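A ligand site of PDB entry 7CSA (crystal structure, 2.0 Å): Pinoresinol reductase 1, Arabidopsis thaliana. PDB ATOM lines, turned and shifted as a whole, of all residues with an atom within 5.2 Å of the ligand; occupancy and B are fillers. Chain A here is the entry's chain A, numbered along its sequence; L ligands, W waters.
NZ of Lys 50 is in salt-bridge range of O17 of the ligand, 2.6 Å away. An oxygen (O15) of the ligand sits at hydrogen-bond distance from the backbone NH (N) of Thr 18 (2.8 Å). OG1 of Thr 18 sits at hydrogen-bond distance from O15 of the ligand, 2.6 Å away. The guanidinium group (NH2) of Arg 41 is in salt-bridge range of an oxygen (O17) of the ligand (2.7 Å). The backbone carbonyl oxygen (O) of Ser 121 sits at hydrogen-bond distance from an oxygen (O12) of the ligand (3.2 Å). O12 of the ligand is in hydrogen-bond range of OG of Ser 121, 2.8 Å away. O4 of the ligand sits at hydrogen-bond distance from N of Ser 90 (3.0 Å). OG of Ser 90 is in hydrogen-bond range of O1 of the ligand (2.9 Å). The backbone NH of Tyr 20 sits at hydrogen-bond distance from an oxygen (O2) of the ligand (2.9 Å). O8 of the ligand lies within hydrogen-bond range of N of Ile 21. O13 of the ligand is in hydrogen-bond range of NZ of Lys 144 (3.1 Å). N of Gly 19 lies within hydrogen-bond range of O5 of the ligand. O12 of the ligand lies within hydrogen-bond range of O of Glu 122 (3.2 Å). N of Ala 17 is in hydrogen-bond range of O15 of the ligand (3.5 Å).
The side-chain amino group (NZ) of Lys 50 sits at hydrogen-bond distance from the side-chain hydroxyl (OG1) of Thr 18, at 2.8 Å. The side-chain hydroxyl (OG) of Ser 121 lies within hydrogen-bond range of the backbone carbonyl oxygen (O) of Met 89. OG of Ser 90 lies within hydrogen-bond range of N of Val 92 (3.1 Å). O of Ser 90 sits close to OD1 of Asn 98 (3.4 Å). The side-chain amino group (NZ) of Lys 144 sits at hydrogen-bond distance from the backbone carbonyl oxygen (O) of Glu 122 (3.0 Å).
The side-chain sulfur (SD) of Met 89 lies close to a nitrogen (N1) of the ligand, at 3.5 Å. The backbone carbonyl oxygen of Phe 123 sits close to an oxygen (O14) of the ligand (2.9 Å). O of Ala 164 lies close to O14 of the ligand (2.9 Å). N of Phe 166 sits close to N7 of the ligand, 2.8 Å away. CA of Gly 16 touches O6 of the ligand, 3.3 Å away. Ile 44 touches the ligand. Phe 69 touches the ligand. Ala 88 touches the ligand (O to C1, 3.3 Å). Gly 91 touches the ligand (N to C13, 3.9 Å). Val 92 touches the ligand (CG1 to O1, 3.7 Å). Ile 99 touches the ligand (CD1 to O12, 3.98 Å). CG1 of Val 101 touches N4 of the ligand, at 3.97 Å. Gly 124 touches the ligand. CA of Cys 165 touches N7 of the ligand, at 3.6 Å. Phe 170 touches the ligand. Hydrophobic or aromatic side chains that line the ligand: Tyr 20, Ile 21, Ile 44, Phe 69, Met 89, Val 92, Ile 99, Val 101, Phe 123, Phe 166 and Phe 170. The nearest printed residue that does not touch the ligand is Leu 39 (4.2 Å).
Water W4 bridges O9 of the ligand (2.5 Å) and OH of Tyr 169 (3.0 Å). Water W12 lies within hydrogen-bond range of O16 of the ligand (2.6 Å), O of Leu 39 (2.6 Å), N of Gly 16 (2.8 Å) and N of Ala 17 (2.9 Å). Water W2 lies within hydrogen-bond range of an oxygen (O1) of the ligand and the side-chain hydroxyl of Ser 90. Water W9 lies within hydrogen-bond range of the backbone NH of Arg 41, an oxygen (O16) of the ligand and the backbone carbonyl oxygen of Leu 39. Water W3 bridges a nitrogen (N5) of the ligand and the guanidinium group of Arg 41. Water W10 lies within hydrogen-bond range of the backbone NH (N) of Gly 91, an oxygen (O9) of the ligand, the backbone NH (N) of Val 92 and the side-chain hydroxyl (OG) of Ser 90.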
ATOM      1  N   GLY A  16     -10.152 -12.886 -36.156  1.00  0.00           N
ATOM      2  CA  GLY A  16      -9.982 -13.268 -34.779  1.00  0.00           C
ATOM      3  C   GLY A  16      -8.706 -14.039 -34.512  1.00  0.00           C
ATOM      4  O   GLY A  16      -8.671 -14.876 -33.591  1.00  0.00           O
ATOM      5  N   ALA A  17      -7.654 -13.784 -35.297  1.00  0.00           N
ATOM      6  CA  ALA A  17      -6.443 -14.583 -35.312  1.00  0.00           C
ATOM      7  C   ALA A  17      -5.655 -14.530 -34.015  1.00  0.00           C
ATOM      8  O   ALA A  17      -4.851 -15.438 -33.766  1.00  0.00           O
ATOM      9  CB  ALA A  17      -5.557 -14.132 -36.487  1.00  0.00           C
ATOM     10  N   THR A  18      -5.826 -13.500 -33.178  1.00  0.00           N
ATOM     11  CA  THR A  18      -5.131 -13.475 -31.901  1.00  0.00           C
ATOM     12  C   THR A  18      -6.021 -13.888 -30.750  1.00  0.00           C
ATOM     13  O   THR A  18      -5.598 -13.795 -29.597  1.00  0.00           O
ATOM     14  CB  THR A  18      -4.481 -12.103 -31.608  1.00  0.00           C
ATOM     15  OG1 THR A  18      -5.480 -11.101 -31.322  1.00  0.00           O
ATOM     16  CG2 THR A  18      -3.577 -11.644 -32.768  1.00  0.00           C
ATOM     17  N   GLY A  19      -7.210 -14.414 -31.041  1.00  0.00           N
ATOM     18  CA  GLY A  19      -8.092 -14.881 -29.992  1.00  0.00           C
ATOM     19  C   GLY A  19      -7.592 -16.164 -29.315  1.00  0.00           C
ATOM     20  O   GLY A  19      -6.608 -16.789 -29.710  1.00  0.00           O
ATOM     21  N   TYR A  20      -8.321 -16.571 -28.267  1.00  0.00           N
ATOM     22  CA  TYR A  20      -7.934 -17.749 -27.503  1.00  0.00           C
ATOM     23  C   TYR A  20      -8.019 -19.014 -28.361  1.00  0.00           C
ATOM     24  O   TYR A  20      -7.056 -19.772 -28.494  1.00  0.00           O
ATOM     25  CB  TYR A  20      -8.802 -17.902 -26.250  1.00  0.00           C
ATOM     26  CG  TYR A  20      -8.442 -19.118 -25.452  1.00  0.00           C
ATOM     27  CD1 TYR A  20      -7.301 -19.136 -24.656  1.00  0.00           C
ATOM     28  CD2 TYR A  20      -9.200 -20.286 -25.524  1.00  0.00           C
ATOM     29  CE1 TYR A  20      -6.939 -20.269 -23.921  1.00  0.00           C
ATOM     30  CE2 TYR A  20      -8.862 -21.423 -24.791  1.00  0.00           C
ATOM     31  CZ  TYR A  20      -7.721 -21.409 -23.998  1.00  0.00           C
ATOM     32  OH  TYR A  20      -7.378 -22.519 -23.280  1.00  0.00           O
ATOM     33  N   ILE A  21      -9.190 -19.282 -28.928  1.00  0.00           N
ATOM     34  CA  ILE A  21      -9.232 -20.363 -29.914  1.00  0.00           C
ATOM     35  C   ILE A  21      -8.671 -19.891 -31.265  1.00  0.00           C
ATOM     36  O   ILE A  21      -8.167 -20.712 -32.038  1.00  0.00           O
ATOM     37  CB  ILE A  21     -10.654 -20.937 -30.107  1.00  0.00           C
ATOM     38  CG1 ILE A  21     -10.599 -22.340 -30.753  1.00  0.00           C
ATOM     39  CG2 ILE A  21     -11.485 -19.989 -30.994  1.00  0.00           C
ATOM     40  CD1 ILE A  21     -10.019 -23.421 -29.848  1.00  0.00           C
ATOM     41  N   GLY A  22      -8.722 -18.592 -31.557  1.00  0.00           N
ATOM     42  CA  GLY A  22      -8.329 -18.149 -32.883  1.00  0.00           C
ATOM     43  C   GLY A  22      -6.846 -18.368 -33.150  1.00  0.00           C
ATOM     44  O   GLY A  22      -6.459 -18.782 -34.246  1.00  0.00           O
ATOM     45  N   LEU A  39      -6.286 -11.691 -40.480  1.00  0.00           N
ATOM     46  CA  LEU A  39      -6.759 -10.305 -40.503  1.00  0.00           C
ATOM     47  C   LEU A  39      -6.118  -9.544 -39.352  1.00  0.00           C
ATOM     48  O   LEU A  39      -6.441  -9.796 -38.183  1.00  0.00           O
ATOM     49  CB  LEU A  39      -8.280 -10.239 -40.418  1.00  0.00           C
ATOM     50  CG  LEU A  39      -8.876  -8.841 -40.668  1.00  0.00           C
ATOM     51  CD1 LEU A  39      -8.866  -8.530 -42.177  1.00  0.00           C
ATOM     52  CD2 LEU A  39     -10.295  -8.778 -40.078  1.00  0.00           C
ATOM     53  N   ARG A  41      -6.137  -6.110 -37.504  1.00  0.00           N
ATOM     54  CA  ARG A  41      -6.966  -4.901 -37.514  1.00  0.00           C
ATOM     55  C   ARG A  41      -6.151  -3.725 -36.998  1.00  0.00           C
ATOM     56  O   ARG A  41      -5.358  -3.874 -36.060  1.00  0.00           O
ATOM     57  CB  ARG A  41      -8.210  -5.104 -36.655  1.00  0.00           C
ATOM     58  CG  ARG A  41      -8.976  -6.395 -37.037  1.00  0.00           C
ATOM     59  CD  ARG A  41     -10.191  -6.688 -36.156  1.00  0.00           C
ATOM     60  NE  ARG A  41      -9.802  -7.031 -34.788  1.00  0.00           N
ATOM     61  CZ  ARG A  41     -10.047  -6.262 -33.721  1.00  0.00           C
ATOM     62  NH1 ARG A  41     -10.682  -5.102 -33.839  1.00  0.00           N
ATOM     63  NH2 ARG A  41      -9.665  -6.680 -32.522  1.00  0.00           N
ATOM     64  N   ILE A  44      -5.884  -2.734 -32.999  1.00  0.00           N
ATOM     65  CA  ILE A  44      -5.083  -3.387 -31.967  1.00  0.00           C
ATOM     66  C   ILE A  44      -3.605  -3.009 -32.075  1.00  0.00           C
ATOM     67  O   ILE A  44      -2.737  -3.703 -31.512  1.00  0.00           O
ATOM     68  CB  ILE A  44      -5.265  -4.921 -31.978  1.00  0.00           C
ATOM     69  CG1 ILE A  44      -4.978  -5.521 -33.359  1.00  0.00           C
ATOM     70  CG2 ILE A  44      -6.657  -5.306 -31.505  1.00  0.00           C
ATOM     71  CD1 ILE A  44      -3.493  -5.626 -33.692  1.00  0.00           C
ATOM     72  N   LYS A  50      -0.853  -8.760 -29.132  1.00  0.00           N
ATOM     73  CA  LYS A  50      -1.455  -9.062 -30.429  1.00  0.00           C
ATOM     74  C   LYS A  50      -0.494  -8.756 -31.580  1.00  0.00           C
ATOM     75  O   LYS A  50      -0.355  -9.552 -32.516  1.00  0.00           O
ATOM     76  CB  LYS A  50      -2.773  -8.285 -30.578  1.00  0.00           C
ATOM     77  CG  LYS A  50      -3.847  -8.764 -29.615  1.00  0.00           C
ATOM     78  CD  LYS A  50      -5.051  -7.857 -29.635  1.00  0.00           C
ATOM     79  CE  LYS A  50      -6.224  -8.501 -28.898  1.00  0.00           C
ATOM     80  NZ  LYS A  50      -7.054  -9.335 -29.804  1.00  0.00           N
ATOM     81  N   PHE A  54       1.051 -11.587 -34.301  1.00  0.00           N
ATOM     82  CA  PHE A  54       1.040 -11.472 -35.751  1.00  0.00           C
ATOM     83  C   PHE A  54       2.445 -11.621 -36.318  1.00  0.00           C
ATOM     84  O   PHE A  54       2.634 -12.261 -37.360  1.00  0.00           O
ATOM     85  CB  PHE A  54       0.420 -10.139 -36.207  1.00  0.00           C
ATOM     86  CG  PHE A  54      -1.097 -10.139 -36.180  1.00  0.00           C
ATOM     87  CD1 PHE A  54      -1.824 -10.898 -37.084  1.00  0.00           C
ATOM     88  CD2 PHE A  54      -1.789  -9.370 -35.259  1.00  0.00           C
ATOM     89  CE1 PHE A  54      -3.214 -10.915 -37.052  1.00  0.00           C
ATOM     90  CE2 PHE A  54      -3.185  -9.382 -35.215  1.00  0.00           C
ATOM     91  CZ  PHE A  54      -3.896 -10.142 -36.103  1.00  0.00           C
ATOM     92  N   PHE A  69     -13.201  -3.820 -39.215  1.00  0.00           N
ATOM     93  CA  PHE A  69     -14.635  -4.052 -39.262  1.00  0.00           C
ATOM     94  C   PHE A  69     -15.440  -2.774 -39.477  1.00  0.00           C
ATOM     95  O   PHE A  69     -16.628  -2.848 -39.796  1.00  0.00           O
ATOM     96  CB  PHE A  69     -15.105  -4.736 -37.981  1.00  0.00           C
ATOM     97  CG  PHE A  69     -14.971  -6.223 -38.021  1.00  0.00           C
ATOM     98  CD1 PHE A  69     -16.013  -7.008 -38.477  1.00  0.00           C
ATOM     99  CD2 PHE A  69     -13.808  -6.835 -37.610  1.00  0.00           C
ATOM    100  CE1 PHE A  69     -15.893  -8.383 -38.514  1.00  0.00           C
ATOM    101  CE2 PHE A  69     -13.676  -8.205 -37.651  1.00  0.00           C
ATOM    102  CZ  PHE A  69     -14.724  -8.986 -38.095  1.00  0.00           C
ATOM    103  N   ALA A  88     -13.236 -16.500 -35.456  1.00  0.00           N
ATOM    104  CA  ALA A  88     -13.094 -16.833 -34.044  1.00  0.00           C
ATOM    105  C   ALA A  88     -13.473 -15.638 -33.181  1.00  0.00           C
ATOM    106  O   ALA A  88     -12.904 -15.414 -32.108  1.00  0.00           O
ATOM    107  CB  ALA A  88     -11.668 -17.303 -33.740  1.00  0.00           C
ATOM    108  N   MET A  89     -14.452 -14.846 -33.637  1.00  0.00           N
ATOM    109  CA  MET A  89     -14.895 -13.686 -32.887  1.00  0.00           C
ATOM    110  C   MET A  89     -15.214 -14.052 -31.434  1.00  0.00           C
ATOM    111  O   MET A  89     -15.753 -15.119 -31.153  1.00  0.00           O
ATOM    112  CB  MET A  89     -16.138 -13.063 -33.527  1.00  0.00           C
ATOM    113  CG  MET A  89     -16.768 -12.009 -32.635  1.00  0.00           C
ATOM    114  SD  MET A  89     -15.738 -10.529 -32.660  1.00  0.00           S
ATOM    115  CE  MET A  89     -15.760 -10.208 -34.424  1.00  0.00           C
ATOM    116  N   SER A  90     -14.901 -13.133 -30.525  1.00  0.00           N
ATOM    117  CA  SER A  90     -15.150 -13.368 -29.107  1.00  0.00           C
ATOM    118  C   SER A  90     -16.641 -13.556 -28.815  1.00  0.00           C
ATOM    119  O   SER A  90     -17.512 -13.015 -29.508  1.00  0.00           O
ATOM    120  CB  SER A  90     -14.635 -12.197 -28.277  1.00  0.00           C
ATOM    121  OG  SER A  90     -14.880 -12.443 -26.912  1.00  0.00           O
ATOM    122  N   GLY A  91     -16.918 -14.325 -27.763  1.00  0.00           N
ATOM    123  CA  GLY A  91     -18.234 -14.424 -27.187  1.00  0.00           C
ATOM    124  C   GLY A  91     -18.425 -13.783 -25.829  1.00  0.00           C
ATOM    125  O   GLY A  91     -19.503 -13.931 -25.237  1.00  0.00           O
ATOM    126  N   VAL A  92     -17.437 -13.060 -25.286  1.00  0.00           N
ATOM    127  CA  VAL A  92     -17.547 -12.729 -23.867  1.00  0.00           C
ATOM    128  C   VAL A  92     -18.474 -11.524 -23.625  1.00  0.00           C
ATOM    129  O   VAL A  92     -19.207 -11.513 -22.621  1.00  0.00           O
ATOM    130  CB  VAL A  92     -16.171 -12.523 -23.189  1.00  0.00           C
ATOM    131  CG1 VAL A  92     -15.073 -13.338 -23.883  1.00  0.00           C
ATOM    132  CG2 VAL A  92     -15.808 -11.046 -23.081  1.00  0.00           C
ATOM    133  N   ASN A  98     -20.751  -8.631 -29.355  1.00  0.00           N
ATOM    134  CA  ASN A  98     -19.584  -8.838 -30.199  1.00  0.00           C
ATOM    135  C   ASN A  98     -19.769 -10.038 -31.150  1.00  0.00           C
ATOM    136  O   ASN A  98     -19.226 -10.020 -32.246  1.00  0.00           O
ATOM    137  CB  ASN A  98     -18.278  -8.956 -29.391  1.00  0.00           C
ATOM    138  CG  ASN A  98     -18.400  -9.828 -28.197  1.00  0.00           C
ATOM    139  OD1 ASN A  98     -19.371 -10.581 -28.068  1.00  0.00           O
ATOM    140  ND2 ASN A  98     -17.403  -9.748 -27.293  1.00  0.00           N
ATOM    141  N   ILE A  99     -20.571 -11.050 -30.782  1.00  0.00           N
ATOM    142  CA  ILE A  99     -20.882 -12.090 -31.764  1.00  0.00           C
ATOM    143  C   ILE A  99     -21.503 -11.472 -33.016  1.00  0.00           C
ATOM    144  O   ILE A  99     -21.224 -11.890 -34.141  1.00  0.00           O
ATOM    145  CB  ILE A  99     -21.796 -13.168 -31.155  1.00  0.00           C
ATOM    146  CG1 ILE A  99     -21.015 -14.065 -30.195  1.00  0.00           C
ATOM    147  CG2 ILE A  99     -22.359 -14.067 -32.241  1.00  0.00           C
ATOM    148  CD1 ILE A  99     -20.089 -15.027 -30.926  1.00  0.00           C
ATOM    149  N   VAL A 101     -20.978  -8.588 -34.340  1.00  0.00           N
ATOM    150  CA  VAL A 101     -20.010  -7.929 -35.205  1.00  0.00           C
ATOM    151  C   VAL A 101     -19.747  -8.769 -36.438  1.00  0.00           C
ATOM    152  O   VAL A 101     -19.435  -8.251 -37.516  1.00  0.00           O
ATOM    153  CB  VAL A 101     -18.717  -7.619 -34.407  1.00  0.00           C
ATOM    154  CG1 VAL A 101     -17.657  -7.016 -35.305  1.00  0.00           C
ATOM    155  CG2 VAL A 101     -19.050  -6.708 -33.244  1.00  0.00           C
ATOM    156  N   SER A 121     -18.117 -18.096 -35.763  1.00  0.00           N
ATOM    157  CA  SER A 121     -17.575 -18.332 -34.422  1.00  0.00           C
ATOM    158  C   SER A 121     -18.568 -19.127 -33.588  1.00  0.00           C
ATOM    159  O   SER A 121     -19.404 -18.579 -32.872  1.00  0.00           O
ATOM    160  CB  SER A 121     -17.222 -17.004 -33.748  1.00  0.00           C
ATOM    161  OG  SER A 121     -16.586 -17.236 -32.509  1.00  0.00           O
ATOM    162  N   GLU A 122     -18.445 -20.445 -33.652  1.00  0.00           N
ATOM    163  CA  GLU A 122     -19.333 -21.335 -32.914  1.00  0.00           C
ATOM    164  C   GLU A 122     -18.536 -21.956 -31.779  1.00  0.00           C
ATOM    165  O   GLU A 122     -18.384 -21.321 -30.726  1.00  0.00           O
ATOM    166  CB  GLU A 122     -19.949 -22.369 -33.854  1.00  0.00           C
ATOM    167  CG  GLU A 122     -20.846 -21.746 -34.917  1.00  0.00           C
ATOM    168  CD  GLU A 122     -22.317 -21.864 -34.564  1.00  0.00           C
ATOM    169  OE1 GLU A 122     -22.638 -22.671 -33.663  1.00  0.00           O
ATOM    170  OE2 GLU A 122     -23.143 -21.169 -35.215  1.00  0.00           O
ATOM    171  N   PHE A 123     -18.011 -23.181 -31.936  1.00  0.00           N
ATOM    172  CA  PHE A 123     -17.011 -23.754 -31.047  1.00  0.00           C
ATOM    173  C   PHE A 123     -17.514 -23.941 -29.620  1.00  0.00           C
ATOM    174  O   PHE A 123     -16.723 -23.972 -28.682  1.00  0.00           O
ATOM    175  CB  PHE A 123     -15.747 -22.888 -31.016  1.00  0.00           C
ATOM    176  CG  PHE A 123     -15.149 -22.650 -32.363  1.00  0.00           C
ATOM    177  CD1 PHE A 123     -14.566 -23.703 -33.062  1.00  0.00           C
ATOM    178  CD2 PHE A 123     -15.152 -21.387 -32.918  1.00  0.00           C
ATOM    179  CE1 PHE A 123     -14.016 -23.494 -34.307  1.00  0.00           C
ATOM    180  CE2 PHE A 123     -14.594 -21.158 -34.157  1.00  0.00           C
ATOM    181  CZ  PHE A 123     -14.020 -22.208 -34.854  1.00  0.00           C
ATOM    182  N   GLY A 124     -18.815 -24.094 -29.443  1.00  0.00           N
ATOM    183  CA  GLY A 124     -19.371 -24.317 -28.121  1.00  0.00           C
ATOM    184  C   GLY A 124     -20.641 -25.161 -28.205  1.00  0.00           C
ATOM    185  O   GLY A 124     -20.769 -26.038 -29.050  1.00  0.00           O
ATOM    186  N   MET A 125     -21.583 -24.870 -27.293  1.00  0.00           N
ATOM    187  CA  MET A 125     -22.896 -25.492 -27.346  1.00  0.00           C
ATOM    188  C   MET A 125     -23.584 -25.187 -28.670  1.00  0.00           C
ATOM    189  O   MET A 125     -23.305 -24.168 -29.319  1.00  0.00           O
ATOM    190  CB  MET A 125     -23.741 -24.999 -26.180  1.00  0.00           C
ATOM    191  CG  MET A 125     -23.226 -25.446 -24.818  1.00  0.00           C
ATOM    192  SD  MET A 125     -24.087 -24.613 -23.473  1.00  0.00           S
ATOM    193  CE  MET A 125     -22.959 -23.283 -23.144  1.00  0.00           C
ATOM    194  N   THR A 140     -26.065 -15.451 -25.864  1.00  0.00           N
ATOM    195  CA  THR A 140     -25.020 -15.960 -26.753  1.00  0.00           C
ATOM    196  C   THR A 140     -25.618 -16.747 -27.915  1.00  0.00           C
ATOM    197  O   THR A 140     -25.222 -16.570 -29.077  1.00  0.00           O
ATOM    198  CB  THR A 140     -24.060 -16.840 -25.967  1.00  0.00           C
ATOM    199  OG1 THR A 140     -23.590 -16.116 -24.833  1.00  0.00           O
ATOM    200  CG2 THR A 140     -22.869 -17.231 -26.841  1.00  0.00           C
ATOM    201  N   LYS A 144     -25.563 -16.010 -32.094  1.00  0.00           N
ATOM    202  CA  LYS A 144     -25.019 -16.984 -33.042  1.00  0.00           C
ATOM    203  C   LYS A 144     -26.103 -17.427 -34.027  1.00  0.00           C
ATOM    204  O   LYS A 144     -25.843 -17.568 -35.228  1.00  0.00           O
ATOM    205  CB  LYS A 144     -24.409 -18.170 -32.293  1.00  0.00           C
ATOM    206  CG  LYS A 144     -23.108 -17.798 -31.546  1.00  0.00           C
ATOM    207  CD  LYS A 144     -22.437 -18.982 -30.859  1.00  0.00           C
ATOM    208  CE  LYS A 144     -21.101 -18.566 -30.202  1.00  0.00           C
ATOM    209  NZ  LYS A 144     -20.517 -19.673 -29.369  1.00  0.00           N
ATOM    210  N   ALA A 164     -18.035 -29.232 -27.712  1.00  0.00           N
ATOM    211  CA  ALA A 164     -17.100 -29.615 -26.666  1.00  0.00           C
ATOM    212  C   ALA A 164     -16.731 -28.440 -25.770  1.00  0.00           C
ATOM    213  O   ALA A 164     -16.596 -27.310 -26.249  1.00  0.00           O
ATOM    214  CB  ALA A 164     -15.810 -30.246 -27.261  1.00  0.00           C
ATOM    215  N   CYS A 165     -16.592 -28.722 -24.478  1.00  0.00           N
ATOM    216  CA  CYS A 165     -16.019 -27.789 -23.524  1.00  0.00           C
ATOM    217  C   CYS A 165     -14.532 -27.572 -23.787  1.00  0.00           C
ATOM    218  O   CYS A 165     -13.781 -28.542 -23.978  1.00  0.00           O
ATOM    219  CB  CYS A 165     -16.203 -28.330 -22.105  1.00  0.00           C
ATOM    220  SG  CYS A 165     -17.858 -28.081 -21.419  1.00  0.00           S
ATOM    221  N   PHE A 166     -14.104 -26.310 -23.802  1.00  0.00           N
ATOM    222  CA  PHE A 166     -12.680 -25.994 -23.824  1.00  0.00           C
ATOM    223  C   PHE A 166     -12.027 -26.557 -22.566  1.00  0.00           C
ATOM    224  O   PHE A 166     -12.493 -26.285 -21.451  1.00  0.00           O
ATOM    225  CB  PHE A 166     -12.455 -24.476 -23.878  1.00  0.00           C
ATOM    226  CG  PHE A 166     -12.750 -23.850 -25.232  1.00  0.00           C
ATOM    227  CD1 PHE A 166     -13.298 -24.594 -26.266  1.00  0.00           C
ATOM    228  CD2 PHE A 166     -12.477 -22.497 -25.451  1.00  0.00           C
ATOM    229  CE1 PHE A 166     -13.566 -24.015 -27.498  1.00  0.00           C
ATOM    230  CE2 PHE A 166     -12.751 -21.891 -26.662  1.00  0.00           C
ATOM    231  CZ  PHE A 166     -13.293 -22.648 -27.697  1.00  0.00           C
ATOM    232  N   TYR A 169     -10.946 -24.368 -19.421  1.00  0.00           N
ATOM    233  CA  TYR A 169     -12.005 -23.701 -18.670  1.00  0.00           C
ATOM    234  C   TYR A 169     -12.907 -24.655 -17.899  1.00  0.00           C
ATOM    235  O   TYR A 169     -13.617 -24.193 -17.003  1.00  0.00           O
ATOM    236  CB  TYR A 169     -12.858 -22.856 -19.623  1.00  0.00           C
ATOM    237  CG  TYR A 169     -12.151 -21.563 -20.064  1.00  0.00           C
ATOM    238  CD1 TYR A 169     -11.969 -20.512 -19.171  1.00  0.00           C
ATOM    239  CD2 TYR A 169     -11.693 -21.412 -21.369  1.00  0.00           C
ATOM    240  CE1 TYR A 169     -11.324 -19.331 -19.571  1.00  0.00           C
ATOM    241  CE2 TYR A 169     -11.042 -20.236 -21.781  1.00  0.00           C
ATOM    242  CZ  TYR A 169     -10.875 -19.200 -20.881  1.00  0.00           C
ATOM    243  OH  TYR A 169     -10.229 -18.034 -21.301  1.00  0.00           O
ATOM    244  N   PHE A 170     -12.877 -25.951 -18.212  1.00  0.00           N
ATOM    245  CA  PHE A 170     -13.782 -26.908 -17.566  1.00  0.00           C
ATOM    246  C   PHE A 170     -13.117 -28.202 -17.117  1.00  0.00           C
ATOM    247  O   PHE A 170     -13.686 -28.901 -16.267  1.00  0.00           O
ATOM    248  CB  PHE A 170     -14.974 -27.241 -18.487  1.00  0.00           C
ATOM    249  CG  PHE A 170     -15.828 -26.037 -18.826  1.00  0.00           C
ATOM    250  CD1 PHE A 170     -15.621 -25.337 -20.006  1.00  0.00           C
ATOM    251  CD2 PHE A 170     -16.776 -25.567 -17.930  1.00  0.00           C
ATOM    252  CE1 PHE A 170     -16.387 -24.194 -20.302  1.00  0.00           C
ATOM    253  CE2 PHE A 170     -17.544 -24.442 -18.213  1.00  0.00           C
ATOM    254  CZ  PHE A 170     -17.347 -23.762 -19.399  1.00  0.00           C
HETATM  255  P1  LIG L   1     -11.680 -14.045 -27.425  1.00  0.00           P
HETATM  256  O1  LIG L   1     -12.211 -13.408 -26.182  1.00  0.00           O
HETATM  257  O2  LIG L   1     -10.338 -14.668 -27.268  1.00  0.00           O
HETATM  258  O3  LIG L   1     -11.667 -12.971 -28.681  1.00  0.00           O
HETATM  259  C1  LIG L   1     -11.313 -13.506 -29.901  1.00  0.00           C
HETATM  260  C2  LIG L   1     -11.256 -12.388 -30.975  1.00  0.00           C
HETATM  261  O4  LIG L   1     -12.365 -11.695 -31.011  1.00  0.00           O
HETATM  262  C3  LIG L   1     -10.261 -11.292 -30.580  1.00  0.00           C
HETATM  263  O5  LIG L   1      -8.950 -11.739 -30.653  1.00  0.00           O
HETATM  264  C4  LIG L   1     -10.662 -10.213 -31.592  1.00  0.00           C
HETATM  265  O6  LIG L   1      -9.989 -10.534 -32.850  1.00  0.00           O
HETATM  266  C5  LIG L   1     -11.943 -10.394 -31.787  1.00  0.00           C
HETATM  267  N1  LIG L   1     -12.769  -9.361 -31.189  1.00  0.00           N
HETATM  268  C6  LIG L   1     -13.242  -9.106 -29.955  1.00  0.00           C
HETATM  269  N2  LIG L   1     -13.979  -7.998 -30.014  1.00  0.00           N
HETATM  270  C7  LIG L   1     -13.963  -7.578 -31.284  1.00  0.00           C
HETATM  271  C8  LIG L   1     -14.560  -6.489 -31.858  1.00  0.00           C
HETATM  272  N3  LIG L   1     -15.438  -5.450 -31.256  1.00  0.00           N
HETATM  273  N4  LIG L   1     -14.415  -6.240 -33.151  1.00  0.00           N
HETATM  274  C9  LIG L   1     -13.655  -7.045 -33.931  1.00  0.00           C
HETATM  275  N5  LIG L   1     -13.066  -8.145 -33.374  1.00  0.00           N
HETATM  276  C10 LIG L   1     -13.212  -8.405 -32.028  1.00  0.00           C
HETATM  277  O7  LIG L   1     -12.722 -15.191 -27.927  1.00  0.00           O
HETATM  278  P2  LIG L   1     -12.709 -16.772 -27.561  1.00  0.00           P
HETATM  279  O8  LIG L   1     -11.593 -17.476 -28.252  1.00  0.00           O
HETATM  280  O9  LIG L   1     -12.757 -16.981 -26.082  1.00  0.00           O
HETATM  281  O10 LIG L   1     -14.182 -17.233 -28.171  1.00  0.00           O
HETATM  282  C11 LIG L   1     -14.301 -17.506 -29.547  1.00  0.00           C
HETATM  283  C12 LIG L   1     -15.465 -18.530 -29.729  1.00  0.00           C
HETATM  284  O11 LIG L   1     -15.264 -19.578 -28.974  1.00  0.00           O
HETATM  285  C13 LIG L   1     -16.793 -17.895 -29.281  1.00  0.00           C
HETATM  286  O12 LIG L   1     -17.817 -18.203 -30.141  1.00  0.00           O
HETATM  287  C14 LIG L   1     -16.981 -18.493 -27.885  1.00  0.00           C
HETATM  288  O13 LIG L   1     -18.423 -18.467 -27.453  1.00  0.00           O
HETATM  289  C15 LIG L   1     -16.543 -19.722 -28.036  1.00  0.00           C
HETATM  290  N6  LIG L   1     -16.074 -20.297 -26.794  1.00  0.00           N
HETATM  291  C16 LIG L   1     -16.396 -21.621 -26.510  1.00  0.00           C
HETATM  292  C17 LIG L   1     -15.969 -22.226 -25.220  1.00  0.00           C
HETATM  293  C18 LIG L   1     -16.225 -23.720 -24.991  1.00  0.00           C
HETATM  294  O14 LIG L   1     -16.626 -24.446 -25.873  1.00  0.00           O
HETATM  295  N7  LIG L   1     -15.911 -24.178 -23.671  1.00  0.00           N
HETATM  296  C19 LIG L   1     -15.271 -21.452 -24.078  1.00  0.00           C
HETATM  297  C20 LIG L   1     -14.780 -20.045 -24.538  1.00  0.00           C
HETATM  298  C21 LIG L   1     -15.260 -19.534 -25.897  1.00  0.00           C
HETATM  299  P3  LIG L   1      -8.440  -9.992 -33.155  1.00  0.00           P
HETATM  300  O15 LIG L   1      -7.521 -11.228 -32.981  1.00  0.00           O
HETATM  301  O16 LIG L   1      -8.485  -9.508 -34.572  1.00  0.00           O
HETATM  302  O17 LIG L   1      -8.052  -8.874 -32.196  1.00  0.00           O
HETATM  303  O   HOH W   1     -10.769 -16.662 -30.625  1.00  0.00           O
HETATM  304  O   HOH W   2     -12.255 -10.806 -25.753  1.00  0.00           O
HETATM  305  O   HOH W   3     -11.532  -9.691 -35.335  1.00  0.00           O
HETATM  306  O   HOH W   4     -11.685 -17.670 -23.920  1.00  0.00           O
HETATM  307  O   HOH W   5      -8.322 -13.489 -25.767  1.00  0.00           O
HETATM  308  O   HOH W   6     -15.412 -20.072 -21.088  1.00  0.00           O
HETATM  309  O   HOH W   7     -11.588 -14.404 -23.732  1.00  0.00           O
HETATM  310  O   HOH W   8     -18.845 -18.660 -24.986  1.00  0.00           O
HETATM  311  O   HOH W   9      -6.377  -7.901 -35.607  1.00  0.00           O
HETATM  312  O   HOH W  10     -15.390 -15.624 -25.823  1.00  0.00           O
HETATM  313  O   HOH W  11     -15.442  -3.934 -34.459  1.00  0.00           O
HETATM  314  O   HOH W  12      -7.984 -11.130 -36.521  1.00  0.00           O
